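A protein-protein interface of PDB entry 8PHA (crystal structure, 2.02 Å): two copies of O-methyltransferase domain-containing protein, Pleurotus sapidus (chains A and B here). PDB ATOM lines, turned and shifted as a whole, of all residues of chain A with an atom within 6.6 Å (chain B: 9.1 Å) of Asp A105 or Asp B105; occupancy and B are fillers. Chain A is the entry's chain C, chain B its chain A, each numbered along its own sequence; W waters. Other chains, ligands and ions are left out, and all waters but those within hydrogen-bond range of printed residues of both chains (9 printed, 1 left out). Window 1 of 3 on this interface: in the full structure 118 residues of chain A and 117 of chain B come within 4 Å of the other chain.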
ATOM      1  N   THR A  98     -20.129 -38.450  17.085  1.00  0.00           N
ATOM      2  CA  THR A  98     -19.986 -36.998  17.138  1.00  0.00           C
ATOM      3  C   THR A  98     -18.765 -36.594  17.951  1.00  0.00           C
ATOM      4  O   THR A  98     -18.032 -35.676  17.557  1.00  0.00           O
ATOM      5  CB  THR A  98     -21.252 -36.339  17.703  1.00  0.00           C
ATOM      6  OG1 THR A  98     -22.387 -36.723  16.918  1.00  0.00           O
ATOM      7  CG2 THR A  98     -21.131 -34.789  17.652  1.00  0.00           C
ATOM      8  N   LEU A 100     -15.953 -38.294  18.617  1.00  0.00           N
ATOM      9  CA  LEU A 100     -14.749 -38.589  17.843  1.00  0.00           C
ATOM     10  C   LEU A 100     -14.475 -37.502  16.812  1.00  0.00           C
ATOM     11  O   LEU A 100     -13.338 -37.007  16.681  1.00  0.00           O
ATOM     12  CB  LEU A 100     -14.909 -39.930  17.141  1.00  0.00           C
ATOM     13  CG  LEU A 100     -14.505 -41.185  17.881  1.00  0.00           C
ATOM     14  CD1 LEU A 100     -14.873 -42.365  17.008  1.00  0.00           C
ATOM     15  CD2 LEU A 100     -12.996 -41.135  18.123  1.00  0.00           C
ATOM     16  N   ASN A 101     -15.510 -37.118  16.058  1.00  0.00           N
ATOM     17  CA  ASN A 101     -15.306 -36.037  15.097  1.00  0.00           C
ATOM     18  C   ASN A 101     -14.894 -34.737  15.787  1.00  0.00           C
ATOM     19  O   ASN A 101     -13.976 -34.053  15.316  1.00  0.00           O
ATOM     20  CB  ASN A 101     -16.554 -35.858  14.236  1.00  0.00           C
ATOM     21  CG  ASN A 101     -16.702 -36.991  13.222  1.00  0.00           C
ATOM     22  OD1 ASN A 101     -15.728 -37.681  12.917  1.00  0.00           O
ATOM     23  ND2 ASN A 101     -17.910 -37.202  12.720  1.00  0.00           N
ATOM     24  N   TYR A 102     -15.501 -34.416  16.940  1.00  0.00           N
ATOM     25  CA  TYR A 102     -15.057 -33.245  17.710  1.00  0.00           C
ATOM     26  C   TYR A 102     -13.575 -33.347  18.056  1.00  0.00           C
ATOM     27  O   TYR A 102     -12.817 -32.371  17.933  1.00  0.00           O
ATOM     28  CB  TYR A 102     -15.875 -33.096  18.999  1.00  0.00           C
ATOM     29  CG  TYR A 102     -17.276 -32.540  18.837  1.00  0.00           C
ATOM     30  CD1 TYR A 102     -17.676 -31.894  17.669  1.00  0.00           C
ATOM     31  CD2 TYR A 102     -18.210 -32.670  19.866  1.00  0.00           C
ATOM     32  CE1 TYR A 102     -18.987 -31.397  17.532  1.00  0.00           C
ATOM     33  CE2 TYR A 102     -19.505 -32.169  19.747  1.00  0.00           C
ATOM     34  CZ  TYR A 102     -19.888 -31.539  18.576  1.00  0.00           C
ATOM     35  OH  TYR A 102     -21.171 -31.044  18.460  1.00  0.00           O
ATOM     36  N   SER A 103     -13.144 -34.529  18.505  1.00  0.00           N
ATOM     37  CA  SER A 103     -11.760 -34.699  18.908  1.00  0.00           C
ATOM     38  C   SER A 103     -10.809 -34.500  17.745  1.00  0.00           C
ATOM     39  O   SER A 103      -9.622 -34.239  17.967  1.00  0.00           O
ATOM     40  CB  SER A 103     -11.556 -36.079  19.522  1.00  0.00           C
ATOM     41  OG  SER A 103     -11.456 -37.056  18.509  1.00  0.00           O
ATOM     42  N   MET A 104     -11.289 -34.623  16.506  1.00  0.00           N
ATOM     43  CA  MET A 104     -10.374 -34.438  15.390  1.00  0.00           C
ATOM     44  C   MET A 104     -10.519 -33.086  14.691  1.00  0.00           C
ATOM     45  O   MET A 104      -9.923 -32.884  13.630  1.00  0.00           O
ATOM     46  CB  MET A 104     -10.542 -35.596  14.413  1.00  0.00           C
ATOM     47  CG  MET A 104      -9.769 -36.817  14.913  1.00  0.00           C
ATOM     48  SD  MET A 104     -10.014 -38.283  13.906  1.00  0.00           S
ATOM     49  CE  MET A 104     -11.721 -38.696  14.282  1.00  0.00           C
ATOM     50  N   ASP A 105     -11.219 -32.127  15.307  1.00  0.00           N
ATOM     51  CA  ASP A 105     -11.452 -30.825  14.689  1.00  0.00           C
ATOM     52  C   ASP A 105     -10.220 -29.916  14.733  1.00  0.00           C
ATOM     53  O   ASP A 105     -10.237 -28.850  14.110  1.00  0.00           O
ATOM     54  CB  ASP A 105     -12.651 -30.139  15.362  1.00  0.00           C
ATOM     55  CG  ASP A 105     -13.997 -30.578  14.765  1.00  0.00           C
ATOM     56  OD1 ASP A 105     -14.000 -31.180  13.666  1.00  0.00           O
ATOM     57  OD2 ASP A 105     -15.052 -30.335  15.399  1.00  0.00           O
ATOM     58  N   VAL A 106      -9.164 -30.299  15.457  1.00  0.00           N
ATOM     59  CA  VAL A 106      -7.916 -29.538  15.460  1.00  0.00           C
ATOM     60  C   VAL A 106      -7.193 -29.658  14.113  1.00  0.00           C
ATOM     61  O   VAL A 106      -6.366 -28.795  13.745  1.00  0.00           O
ATOM     62  CB  VAL A 106      -7.072 -30.036  16.657  1.00  0.00           C
ATOM     63  CG1 VAL A 106      -7.026 -31.570  16.659  1.00  0.00           C
ATOM     64  CG2 VAL A 106      -5.680 -29.464  16.654  1.00  0.00           C
ATOM     65  N   LEU A 107      -7.535 -30.692  13.333  1.00  0.00           N
ATOM     66  CA  LEU A 107      -6.738 -31.038  12.160  1.00  0.00           C
ATOM     67  C   LEU A 107      -6.942 -30.060  11.008  1.00  0.00           C
ATOM     68  O   LEU A 107      -5.966 -29.640  10.372  1.00  0.00           O
ATOM     69  CB  LEU A 107      -7.067 -32.456  11.712  1.00  0.00           C
ATOM     70  CG  LEU A 107      -6.818 -33.474  12.824  1.00  0.00           C
ATOM     71  CD1 LEU A 107      -7.207 -34.872  12.377  1.00  0.00           C
ATOM     72  CD2 LEU A 107      -5.343 -33.396  13.228  1.00  0.00           C
ATOM     73  N   VAL A 108      -8.190 -29.672  10.729  1.00  0.00           N
ATOM     74  CA  VAL A 108      -8.424 -28.740   9.625  1.00  0.00           C
ATOM     75  C   VAL A 108      -7.724 -27.413   9.846  1.00  0.00           C
ATOM     76  O   VAL A 108      -7.057 -26.932   8.908  1.00  0.00           O
ATOM     77  CB  VAL A 108      -9.953 -28.561   9.397  1.00  0.00           C
ATOM     78  CG1 VAL A 108     -10.209 -27.249   8.642  1.00  0.00           C
ATOM     79  CG2 VAL A 108     -10.530 -29.743   8.637  1.00  0.00           C
ATOM     80  N   PRO A 109      -7.806 -26.765  11.020  1.00  0.00           N
ATOM     81  CA  PRO A 109      -7.011 -25.542  11.223  1.00  0.00           C
ATOM     82  C   PRO A 109      -5.517 -25.773  11.123  1.00  0.00           C
ATOM     83  O   PRO A 109      -4.795 -24.896  10.618  1.00  0.00           O
ATOM     84  CB  PRO A 109      -7.431 -25.065  12.624  1.00  0.00           C
ATOM     85  CG  PRO A 109      -8.205 -26.194  13.239  1.00  0.00           C
ATOM     86  CD  PRO A 109      -8.799 -26.949  12.099  1.00  0.00           C
ATOM     87  N   SER A 110      -5.022 -26.933  11.574  1.00  0.00           N
ATOM     88  CA  SER A 110      -3.610 -27.233  11.335  1.00  0.00           C
ATOM     89  C   SER A 110      -3.278 -27.224   9.834  1.00  0.00           C
ATOM     90  O   SER A 110      -2.247 -26.679   9.414  1.00  0.00           O
ATOM     91  CB  SER A 110      -3.251 -28.579  11.968  1.00  0.00           C
ATOM     92  OG  SER A 110      -1.931 -28.940  11.629  1.00  0.00           O
ATOM     93  N   THR A 424     -16.804 -19.592  20.996  1.00  0.00           N
ATOM     94  CA  THR A 424     -15.405 -19.698  20.581  1.00  0.00           C
ATOM     95  C   THR A 424     -14.666 -18.386  20.823  1.00  0.00           C
ATOM     96  O   THR A 424     -13.480 -18.392  21.176  1.00  0.00           O
ATOM     97  CB  THR A 424     -15.281 -20.091  19.105  1.00  0.00           C
ATOM     98  OG1 THR A 424     -15.879 -19.081  18.280  1.00  0.00           O
ATOM     99  CG2 THR A 424     -15.939 -21.440  18.834  1.00  0.00           C
ATOM    100  N   THR B  98     -17.363 -19.254   6.802  1.00  0.00           N
ATOM    101  CA  THR B  98     -17.007 -20.657   6.977  1.00  0.00           C
ATOM    102  C   THR B  98     -15.550 -20.815   7.378  1.00  0.00           C
ATOM    103  O   THR B  98     -15.230 -21.566   8.307  1.00  0.00           O
ATOM    104  CB  THR B  98     -17.296 -21.420   5.686  1.00  0.00           C
ATOM    105  OG1 THR B  98     -18.684 -21.280   5.353  1.00  0.00           O
ATOM    106  CG2 THR B  98     -16.955 -22.896   5.846  1.00  0.00           C
ATOM    107  N   MET B  99     -14.646 -20.110   6.686  1.00  0.00           N
ATOM    108  CA  MET B  99     -13.229 -20.276   6.982  1.00  0.00           C
ATOM    109  C   MET B  99     -12.882 -19.760   8.375  1.00  0.00           C
ATOM    110  O   MET B  99     -12.017 -20.331   9.049  1.00  0.00           O
ATOM    111  CB  MET B  99     -12.389 -19.586   5.912  1.00  0.00           C
ATOM    112  CG  MET B  99     -12.482 -20.278   4.547  1.00  0.00           C
ATOM    113  SD  MET B  99     -11.601 -21.847   4.525  1.00  0.00           S
ATOM    114  CE  MET B  99      -9.897 -21.299   4.598  1.00  0.00           C
ATOM    115  N   LEU B 100     -13.558 -18.708   8.835  1.00  0.00           N
ATOM    116  CA  LEU B 100     -13.353 -18.237  10.196  1.00  0.00           C
ATOM    117  C   LEU B 100     -13.757 -19.312  11.202  1.00  0.00           C
ATOM    118  O   LEU B 100     -13.017 -19.609  12.164  1.00  0.00           O
ATOM    119  CB  LEU B 100     -14.147 -16.942  10.398  1.00  0.00           C
ATOM    120  CG  LEU B 100     -13.869 -16.122  11.652  1.00  0.00           C
ATOM    121  CD1 LEU B 100     -12.390 -15.758  11.757  1.00  0.00           C
ATOM    122  CD2 LEU B 100     -14.738 -14.866  11.630  1.00  0.00           C
ATOM    123  N   ASN B 101     -14.923 -19.934  10.975  1.00  0.00           N
ATOM    124  CA  ASN B 101     -15.339 -20.995  11.888  1.00  0.00           C
ATOM    125  C   ASN B 101     -14.376 -22.186  11.850  1.00  0.00           C
ATOM    126  O   ASN B 101     -14.060 -22.760  12.898  1.00  0.00           O
ATOM    127  CB  ASN B 101     -16.773 -21.406  11.589  1.00  0.00           C
ATOM    128  CG  ASN B 101     -17.773 -20.356  12.072  1.00  0.00           C
ATOM    129  OD1 ASN B 101     -17.443 -19.515  12.917  1.00  0.00           O
ATOM    130  ND2 ASN B 101     -18.984 -20.390  11.531  1.00  0.00           N
ATOM    131  N   TYR B 102     -13.871 -22.548  10.662  1.00  0.00           N
ATOM    132  CA  TYR B 102     -12.833 -23.584  10.562  1.00  0.00           C
ATOM    133  C   TYR B 102     -11.609 -23.204  11.384  1.00  0.00           C
ATOM    134  O   TYR B 102     -11.030 -24.040  12.086  1.00  0.00           O
ATOM    135  CB  TYR B 102     -12.405 -23.800   9.102  1.00  0.00           C
ATOM    136  CG  TYR B 102     -13.336 -24.604   8.204  1.00  0.00           C
ATOM    137  CD1 TYR B 102     -14.357 -25.396   8.725  1.00  0.00           C
ATOM    138  CD2 TYR B 102     -13.199 -24.542   6.824  1.00  0.00           C
ATOM    139  CE1 TYR B 102     -15.198 -26.117   7.892  1.00  0.00           C
ATOM    140  CE2 TYR B 102     -14.029 -25.259   5.981  1.00  0.00           C
ATOM    141  CZ  TYR B 102     -15.033 -26.042   6.518  1.00  0.00           C
ATOM    142  OH  TYR B 102     -15.870 -26.743   5.672  1.00  0.00           O
ATOM    143  N   SER B 103     -11.176 -21.941  11.274  1.00  0.00           N
ATOM    144  CA  SER B 103      -9.972 -21.505  11.967  1.00  0.00           C
ATOM    145  C   SER B 103     -10.126 -21.627  13.468  1.00  0.00           C
ATOM    146  O   SER B 103      -9.120 -21.746  14.174  1.00  0.00           O
ATOM    147  CB  SER B 103      -9.629 -20.060  11.606  1.00  0.00           C
ATOM    148  OG  SER B 103     -10.439 -19.164  12.353  1.00  0.00           O
ATOM    149  N   MET B 104     -11.356 -21.623  13.977  1.00  0.00           N
ATOM    150  CA  MET B 104     -11.519 -21.767  15.421  1.00  0.00           C
ATOM    151  C   MET B 104     -11.869 -23.187  15.868  1.00  0.00           C
ATOM    152  O   MET B 104     -12.261 -23.378  17.025  1.00  0.00           O
ATOM    153  CB  MET B 104     -12.563 -20.774  15.923  1.00  0.00           C
ATOM    154  CG  MET B 104     -11.977 -19.373  15.957  1.00  0.00           C
ATOM    155  SD  MET B 104     -13.077 -18.089  16.526  1.00  0.00           S
ATOM    156  CE  MET B 104     -13.923 -17.701  15.008  1.00  0.00           C
ATOM    157  N   ASP B 105     -11.637 -24.198  15.027  1.00  0.00           N
ATOM    158  CA  ASP B 105     -12.045 -25.560  15.372  1.00  0.00           C
ATOM    159  C   ASP B 105     -11.099 -26.260  16.358  1.00  0.00           C
ATOM    160  O   ASP B 105     -11.414 -27.370  16.791  1.00  0.00           O
ATOM    161  CB  ASP B 105     -12.191 -26.408  14.093  1.00  0.00           C
ATOM    162  CG  ASP B 105     -13.613 -26.372  13.500  1.00  0.00           C
ATOM    163  OD1 ASP B 105     -14.561 -25.930  14.188  1.00  0.00           O
ATOM    164  OD2 ASP B 105     -13.780 -26.787  12.330  1.00  0.00           O
ATOM    165  N   VAL B 106      -9.974 -25.644  16.744  1.00  0.00           N
ATOM    166  CA  VAL B 106      -9.079 -26.216  17.760  1.00  0.00           C
ATOM    167  C   VAL B 106      -9.696 -26.141  19.156  1.00  0.00           C
ATOM    168  O   VAL B 106      -9.337 -26.925  20.065  1.00  0.00           O
ATOM    169  CB  VAL B 106      -7.722 -25.473  17.701  1.00  0.00           C
ATOM    170  CG1 VAL B 106      -6.984 -25.521  19.015  1.00  0.00           C
ATOM    171  CG2 VAL B 106      -6.850 -26.038  16.603  1.00  0.00           C
ATOM    172  N   LEU B 107     -10.654 -25.227  19.334  1.00  0.00           N
ATOM    173  CA  LEU B 107     -11.086 -24.837  20.671  1.00  0.00           C
ATOM    174  C   LEU B 107     -11.908 -25.926  21.348  1.00  0.00           C
ATOM    175  O   LEU B 107     -11.726 -26.194  22.542  1.00  0.00           O
ATOM    176  CB  LEU B 107     -11.873 -23.532  20.588  1.00  0.00           C
ATOM    177  CG  LEU B 107     -11.055 -22.421  19.918  1.00  0.00           C
ATOM    178  CD1 LEU B 107     -11.873 -21.152  19.802  1.00  0.00           C
ATOM    179  CD2 LEU B 107      -9.736 -22.161  20.682  1.00  0.00           C
ATOM    180  N   VAL B 108     -12.833 -26.554  20.620  1.00  0.00           N
ATOM    181  CA  VAL B 108     -13.625 -27.624  21.224  1.00  0.00           C
ATOM    182  C   VAL B 108     -12.757 -28.787  21.688  1.00  0.00           C
ATOM    183  O   VAL B 108     -12.919 -29.225  22.840  1.00  0.00           O
ATOM    184  CB  VAL B 108     -14.744 -28.065  20.258  1.00  0.00           C
ATOM    185  CG1 VAL B 108     -15.299 -29.406  20.703  1.00  0.00           C
ATOM    186  CG2 VAL B 108     -15.846 -27.013  20.215  1.00  0.00           C
ATOM    187  N   PRO B 109     -11.835 -29.331  20.880  1.00  0.00           N
ATOM    188  CA  PRO B 109     -10.964 -30.405  21.406  1.00  0.00           C
ATOM    189  C   PRO B 109     -10.146 -29.958  22.599  1.00  0.00           C
ATOM    190  O   PRO B 109      -9.912 -30.750  23.523  1.00  0.00           O
ATOM    191  CB  PRO B 109     -10.052 -30.765  20.228  1.00  0.00           C
ATOM    192  CG  PRO B 109     -10.637 -30.133  19.035  1.00  0.00           C
ATOM    193  CD  PRO B 109     -11.597 -29.059  19.452  1.00  0.00           C
ATOM    194  N   SER B 110      -9.675 -28.706  22.589  1.00  0.00           N
ATOM    195  CA  SER B 110      -8.962 -28.196  23.755  1.00  0.00           C
ATOM    196  C   SER B 110      -9.846 -28.254  24.997  1.00  0.00           C
ATOM    197  O   SER B 110      -9.399 -28.674  26.076  1.00  0.00           O
ATOM    198  CB  SER B 110      -8.489 -26.764  23.488  1.00  0.00           C
ATOM    199  OG  SER B 110      -7.869 -26.202  24.629  1.00  0.00           O
ATOM    200  N   CYS B 111     -11.110 -27.851  24.858  1.00  0.00           N
ATOM    201  CA  CYS B 111     -12.040 -27.889  25.983  1.00  0.00           C
ATOM    202  C   CYS B 111     -12.305 -29.316  26.437  1.00  0.00           C
ATOM    203  O   CYS B 111     -12.391 -29.590  27.643  1.00  0.00           O
ATOM    204  CB  CYS B 111     -13.353 -27.198  25.600  1.00  0.00           C
ATOM    205  SG  CYS B 111     -13.211 -25.399  25.440  1.00  0.00           S
ATOM    206  N   ILE B 112     -12.450 -30.236  25.481  1.00  0.00           N
ATOM    207  CA  ILE B 112     -12.658 -31.640  25.822  1.00  0.00           C
ATOM    208  C   ILE B 112     -11.480 -32.166  26.633  1.00  0.00           C
ATOM    209  O   ILE B 112     -11.658 -32.807  27.681  1.00  0.00           O
ATOM    210  CB  ILE B 112     -12.867 -32.482  24.551  1.00  0.00           C
ATOM    211  CG1 ILE B 112     -14.210 -32.173  23.881  1.00  0.00           C
ATOM    212  CG2 ILE B 112     -12.791 -33.965  24.893  1.00  0.00           C
ATOM    213  CD1 ILE B 112     -14.404 -32.934  22.561  1.00  0.00           C
ATOM    214  N   LEU B 153     -18.830 -23.557  25.892  1.00  0.00           N
ATOM    215  CA  LEU B 153     -18.472 -23.919  24.523  1.00  0.00           C
ATOM    216  C   LEU B 153     -18.823 -25.377  24.242  1.00  0.00           C
ATOM    217  O   LEU B 153     -19.354 -25.697  23.170  1.00  0.00           O
ATOM    218  CB  LEU B 153     -16.991 -23.648  24.242  1.00  0.00           C
ATOM    219  CG  LEU B 153     -16.516 -24.009  22.824  1.00  0.00           C
ATOM    220  CD1 LEU B 153     -17.418 -23.399  21.740  1.00  0.00           C
ATOM    221  CD2 LEU B 153     -15.066 -23.600  22.598  1.00  0.00           C
ATOM    222  N   ASN B 157     -22.201 -27.116  21.824  1.00  0.00           N
ATOM    223  CA  ASN B 157     -22.010 -28.254  20.936  1.00  0.00           C
ATOM    224  C   ASN B 157     -22.574 -29.559  21.499  1.00  0.00           C
ATOM    225  O   ASN B 157     -22.126 -30.638  21.094  1.00  0.00           O
ATOM    226  CB  ASN B 157     -20.532 -28.407  20.587  1.00  0.00           C
ATOM    227  CG  ASN B 157     -20.070 -27.350  19.594  1.00  0.00           C
ATOM    228  OD1 ASN B 157     -20.268 -27.493  18.389  1.00  0.00           O
ATOM    229  ND2 ASN B 157     -19.460 -26.287  20.097  1.00  0.00           N
ATOM    230  N   LYS B 190      -6.711 -38.379  21.553  1.00  0.00           N
ATOM    231  CA  LYS B 190      -6.799 -37.520  20.375  1.00  0.00           C
ATOM    232  C   LYS B 190      -6.852 -36.041  20.732  1.00  0.00           C
ATOM    233  O   LYS B 190      -6.407 -35.206  19.935  1.00  0.00           O
ATOM    234  CB  LYS B 190      -8.022 -37.878  19.537  1.00  0.00           C
ATOM    235  CG  LYS B 190      -7.845 -39.093  18.662  1.00  0.00           C
ATOM    236  CD  LYS B 190      -9.065 -39.250  17.739  1.00  0.00           C
ATOM    237  CE  LYS B 190      -8.862 -40.414  16.787  1.00  0.00           C
ATOM    238  NZ  LYS B 190      -7.632 -40.262  15.962  1.00  0.00           N
ATOM    239  N   THR B 191      -7.400 -35.680  21.896  1.00  0.00           N
ATOM    240  CA  THR B 191      -7.408 -34.278  22.299  1.00  0.00           C
ATOM    241  C   THR B 191      -6.244 -33.905  23.213  1.00  0.00           C
ATOM    242  O   THR B 191      -6.074 -32.720  23.525  1.00  0.00           O
ATOM    243  CB  THR B 191      -8.723 -33.938  23.005  1.00  0.00           C
ATOM    244  OG1 THR B 191      -8.814 -34.682  24.229  1.00  0.00           O
ATOM    245  CG2 THR B 191      -9.907 -34.264  22.106  1.00  0.00           C
ATOM    246  N   THR B 199       0.470 -31.471  16.177  1.00  0.00           N
ATOM    247  CA  THR B 199       0.084 -30.440  15.226  1.00  0.00           C
ATOM    248  C   THR B 199       0.722 -29.090  15.527  1.00  0.00           C
ATOM    249  O   THR B 199       0.298 -28.082  14.963  1.00  0.00           O
ATOM    250  CB  THR B 199      -1.441 -30.296  15.157  1.00  0.00           C
ATOM    251  OG1 THR B 199      -1.981 -30.172  16.476  1.00  0.00           O
ATOM    252  CG2 THR B 199      -2.064 -31.512  14.451  1.00  0.00           C
ATOM    253  N   ARG B 417     -17.943 -33.911   3.938  1.00  0.00           N
ATOM    254  CA  ARG B 417     -17.705 -34.046   5.371  1.00  0.00           C
ATOM    255  C   ARG B 417     -18.275 -35.341   5.938  1.00  0.00           C
ATOM    256  O   ARG B 417     -17.776 -35.830   6.964  1.00  0.00           O
ATOM    257  CB  ARG B 417     -18.270 -32.847   6.128  1.00  0.00           C
ATOM    258  CG  ARG B 417     -17.489 -32.621   7.423  1.00  0.00           C
ATOM    259  CD  ARG B 417     -17.965 -31.420   8.138  1.00  0.00           C
ATOM    260  NE  ARG B 417     -17.606 -30.188   7.452  1.00  0.00           N
ATOM    261  CZ  ARG B 417     -18.233 -29.044   7.665  1.00  0.00           C
ATOM    262  NH1 ARG B 417     -19.250 -28.969   8.507  1.00  0.00           N
ATOM    263  NH2 ARG B 417     -17.840 -27.953   7.013  1.00  0.00           N
ATOM    264  N   ALA B 420     -15.508 -37.765   6.651  1.00  0.00           N
ATOM    265  CA  ALA B 420     -14.344 -37.060   7.191  1.00  0.00           C
ATOM    266  C   ALA B 420     -13.298 -37.990   7.795  1.00  0.00           C
ATOM    267  O   ALA B 420     -12.093 -37.751   7.648  1.00  0.00           O
ATOM    268  CB  ALA B 420     -14.795 -36.033   8.231  1.00  0.00           C
ATOM    269  N   THR B 424      -9.382 -37.310   8.014  1.00  0.00           N
ATOM    270  CA  THR B 424      -8.755 -37.003   9.297  1.00  0.00           C
ATOM    271  C   THR B 424      -7.910 -38.177   9.775  1.00  0.00           C
ATOM    272  O   THR B 424      -6.931 -37.972  10.497  1.00  0.00           O
ATOM    273  CB  THR B 424      -9.792 -36.625  10.365  1.00  0.00           C
ATOM    274  OG1 THR B 424     -10.725 -37.698  10.544  1.00  0.00           O
ATOM    275  CG2 THR B 424     -10.562 -35.349   9.969  1.00  0.00           C
ATOM    276  N   TYR B 427      -4.447 -37.758   7.810  1.00  0.00           N
ATOM    277  CA  TYR B 427      -3.666 -36.681   8.416  1.00  0.00           C
ATOM    278  C   TYR B 427      -3.198 -37.063   9.814  1.00  0.00           C
ATOM    279  O   TYR B 427      -2.049 -36.788  10.184  1.00  0.00           O
ATOM    280  CB  TYR B 427      -4.464 -35.373   8.441  1.00  0.00           C
ATOM    281  CG  TYR B 427      -3.603 -34.170   8.792  1.00  0.00           C
ATOM    282  CD1 TYR B 427      -2.428 -33.909   8.091  1.00  0.00           C
ATOM    283  CD2 TYR B 427      -3.975 -33.287   9.795  1.00  0.00           C
ATOM    284  CE1 TYR B 427      -1.644 -32.811   8.395  1.00  0.00           C
ATOM    285  CE2 TYR B 427      -3.204 -32.184  10.100  1.00  0.00           C
ATOM    286  CZ  TYR B 427      -2.045 -31.952   9.397  1.00  0.00           C
ATOM    287  OH  TYR B 427      -1.295 -30.851   9.703  1.00  0.00           O
ATOM    288  N   THR B 428      -4.054 -37.736  10.595  1.00  0.00           N
ATOM    289  CA  THR B 428      -3.605 -38.185  11.910  1.00  0.00           C
ATOM    290  C   THR B 428      -2.395 -39.104  11.776  1.00  0.00           C
ATOM    291  O   THR B 428      -1.368 -38.905  12.443  1.00  0.00           O
ATOM    292  CB  THR B 428      -4.739 -38.887  12.657  1.00  0.00           C
ATOM    293  OG1 THR B 428      -5.772 -37.940  12.957  1.00  0.00           O
ATOM    294  CG2 THR B 428      -4.222 -39.529  13.957  1.00  0.00           C
HETATM  295  O   HOH W   1     -18.551 -36.866   9.422  1.00  0.00           O
HETATM  296  O   HOH W   2     -16.518 -20.290  15.835  1.00  0.00           O
HETATM  297  O   HOH W   3      -0.293 -27.131  12.409  1.00  0.00           O
HETATM  298  O   HOH W   4      -7.794 -41.057  13.267  1.00  0.00           O
HETATM  299  O   HOH W   5     -14.616 -27.781  16.887  1.00  0.00           O
HETATM  300  O   HOH W   6     -12.739 -28.868  11.540  1.00  0.00           O
HETATM  301  O   HOH W   7     -10.240 -40.533  11.734  1.00  0.00           O
HETATM  302  O   HOH W   8     -13.062 -37.002  11.744  1.00  0.00           O
HETATM  303  O   HOH W   9     -15.224 -15.946  17.670  1.00  0.00           O
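SD of Met B104 lies within hydrogen-bond range of OG1 of Thr A424, 3.5 Å away.
The backbone carbonyl oxygen of Asn B157 sits at hydrogen-bond distance from the side-chain hydroxyl of Tyr A102 (2.8 Å).
NZ of Lys B190 sits at hydrogen-bond distance from SD of Met A104.
The side-chain hydroxyl of Thr B424 sits at hydrogen-bond distance from the side-chain sulfur of Met A104 (3.5 Å).
The side-chain hydroxyl of Tyr B427 sits at hydrogen-bond distance from the side-chain hydroxyl of Ser A110 (2.8 Å).
O of Asp A105 sits close to O of Asp B105.
The backbone carbonyl oxygen (O) of Leu B107 sits at hydrogen-bond distance from the side-chain sulfur (SG) of Cys B111 (3.4 Å).
The backbone carbonyl oxygen (O) of Leu B153 lies within hydrogen-bond range of the side-chain amide nitrogen (ND2) of Asn B157 (3.1 Å).
The backbone carbonyl oxygen (O) of Thr B424 sits at hydrogen-bond distance from the side-chain hydroxyl (OG1) of Thr B428 (2.7 Å).
The side-chain hydroxyl (OG) of Ser A103 sits at hydrogen-bond distance from the backbone carbonyl oxygen (O) of Leu A100, at 2.6 Å.
Pro B109 touches Tyr A102.
Ile B112 touches Tyr A102.
CD of Lys B190 touches OG of Ser A103, 3.3 Å away.
CB of Ser A103 touches CG2 of Thr B191, at 3.6 Å.
N of Val A106 touches O of Asp B105 (3.9 Å).
Val A106 touches Val B106.
Pro B109 touches Val A106.
Val A106 touches Thr B199 (CG2 to OG1, 3.8 Å).
CD1 of Leu A107 touches OG1 of Thr B428, 3.4 Å away.
Pro A109 touches Val B106 (CG to CG2, 3.6 Å).
Of the printed residues of chain B, Tyr A102 touches Pro B109, Ile B112 and Asn B157.
Asp A105 touches just one residue of chain B: Asp B105.
Of chain B, only Asp B105 (3.9 Å), Val B106 (3.6 Å), Pro B109 (3.9 Å) and Thr B199 (3.8 Å) come within 4 Å of Val A106.
Leu B100 touches none of the printed residues of chain A.
Asn B101 touches none of the printed residues of chain A.
Of chain A, only Asp A105 (3.1 Å), Val A106 (3.9 Å) and Pro A109 (3.97 Å) come within 4 Å of Asp B105.
Of the printed residues of chain A, Tyr B427 touches Leu A107 (3.7 Å) and Ser A110 (2.8 Å).
The nearest residue of chain B that does not touch Asp A105 is Val B106 (4.2 Å).
The nearest printed residue of chain B that does not touch Ser A110 is Val B106 (5.4 Å).
Of the 25 printed residues of chain B, 15 touch a printed residue of chain A.
Hydrophobic or aromatic side chains of chain B within 4 Å of the printed part of chain A: Met B104, Val B106, Leu B107, Pro B109, Ile B112, Leu B153 and Tyr B427.
Of the 13 printed residues of chain A, 9 touch a printed residue of chain B.
Tyr A102 touches Pro B109, and with the chains exchanged Pro A109 touches Tyr B102.
Val A106 touches Asp B105, but with the chains exchanged Asp A105 does not touch Val B106 (4.2 Å).
Leu A107 touches Thr B424, and with the chains exchanged Thr A424 touches Leu B107.
Pro A109 touches Asp B105, but with the chains exchanged Asp A105 does not touch Pro B109 (4.2 Å).
Water W3 bridges the side-chain hydroxyl of Ser A110 (2.6 Å) and the backbone carbonyl oxygen of Thr B199 (2.8 Å).
Water W2 lies within hydrogen-bond range of OG1 of Thr A424 and OD1 of Asn B101.
Water W4 bridges NZ of Lys B190 (2.8 Å) and SD of Met A104 (3.6 Å).
Water W7 bridges the side-chain hydroxyl (OG1) of Thr B424 (3.1 Å) and the side-chain sulfur (SD) of Met A104 (3.1 Å).
Water W9 bridges the side-chain sulfur (SD) of Met B104 (3.2 Å) and the side-chain hydroxyl (OG1) of Thr A424 (3.3 Å).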
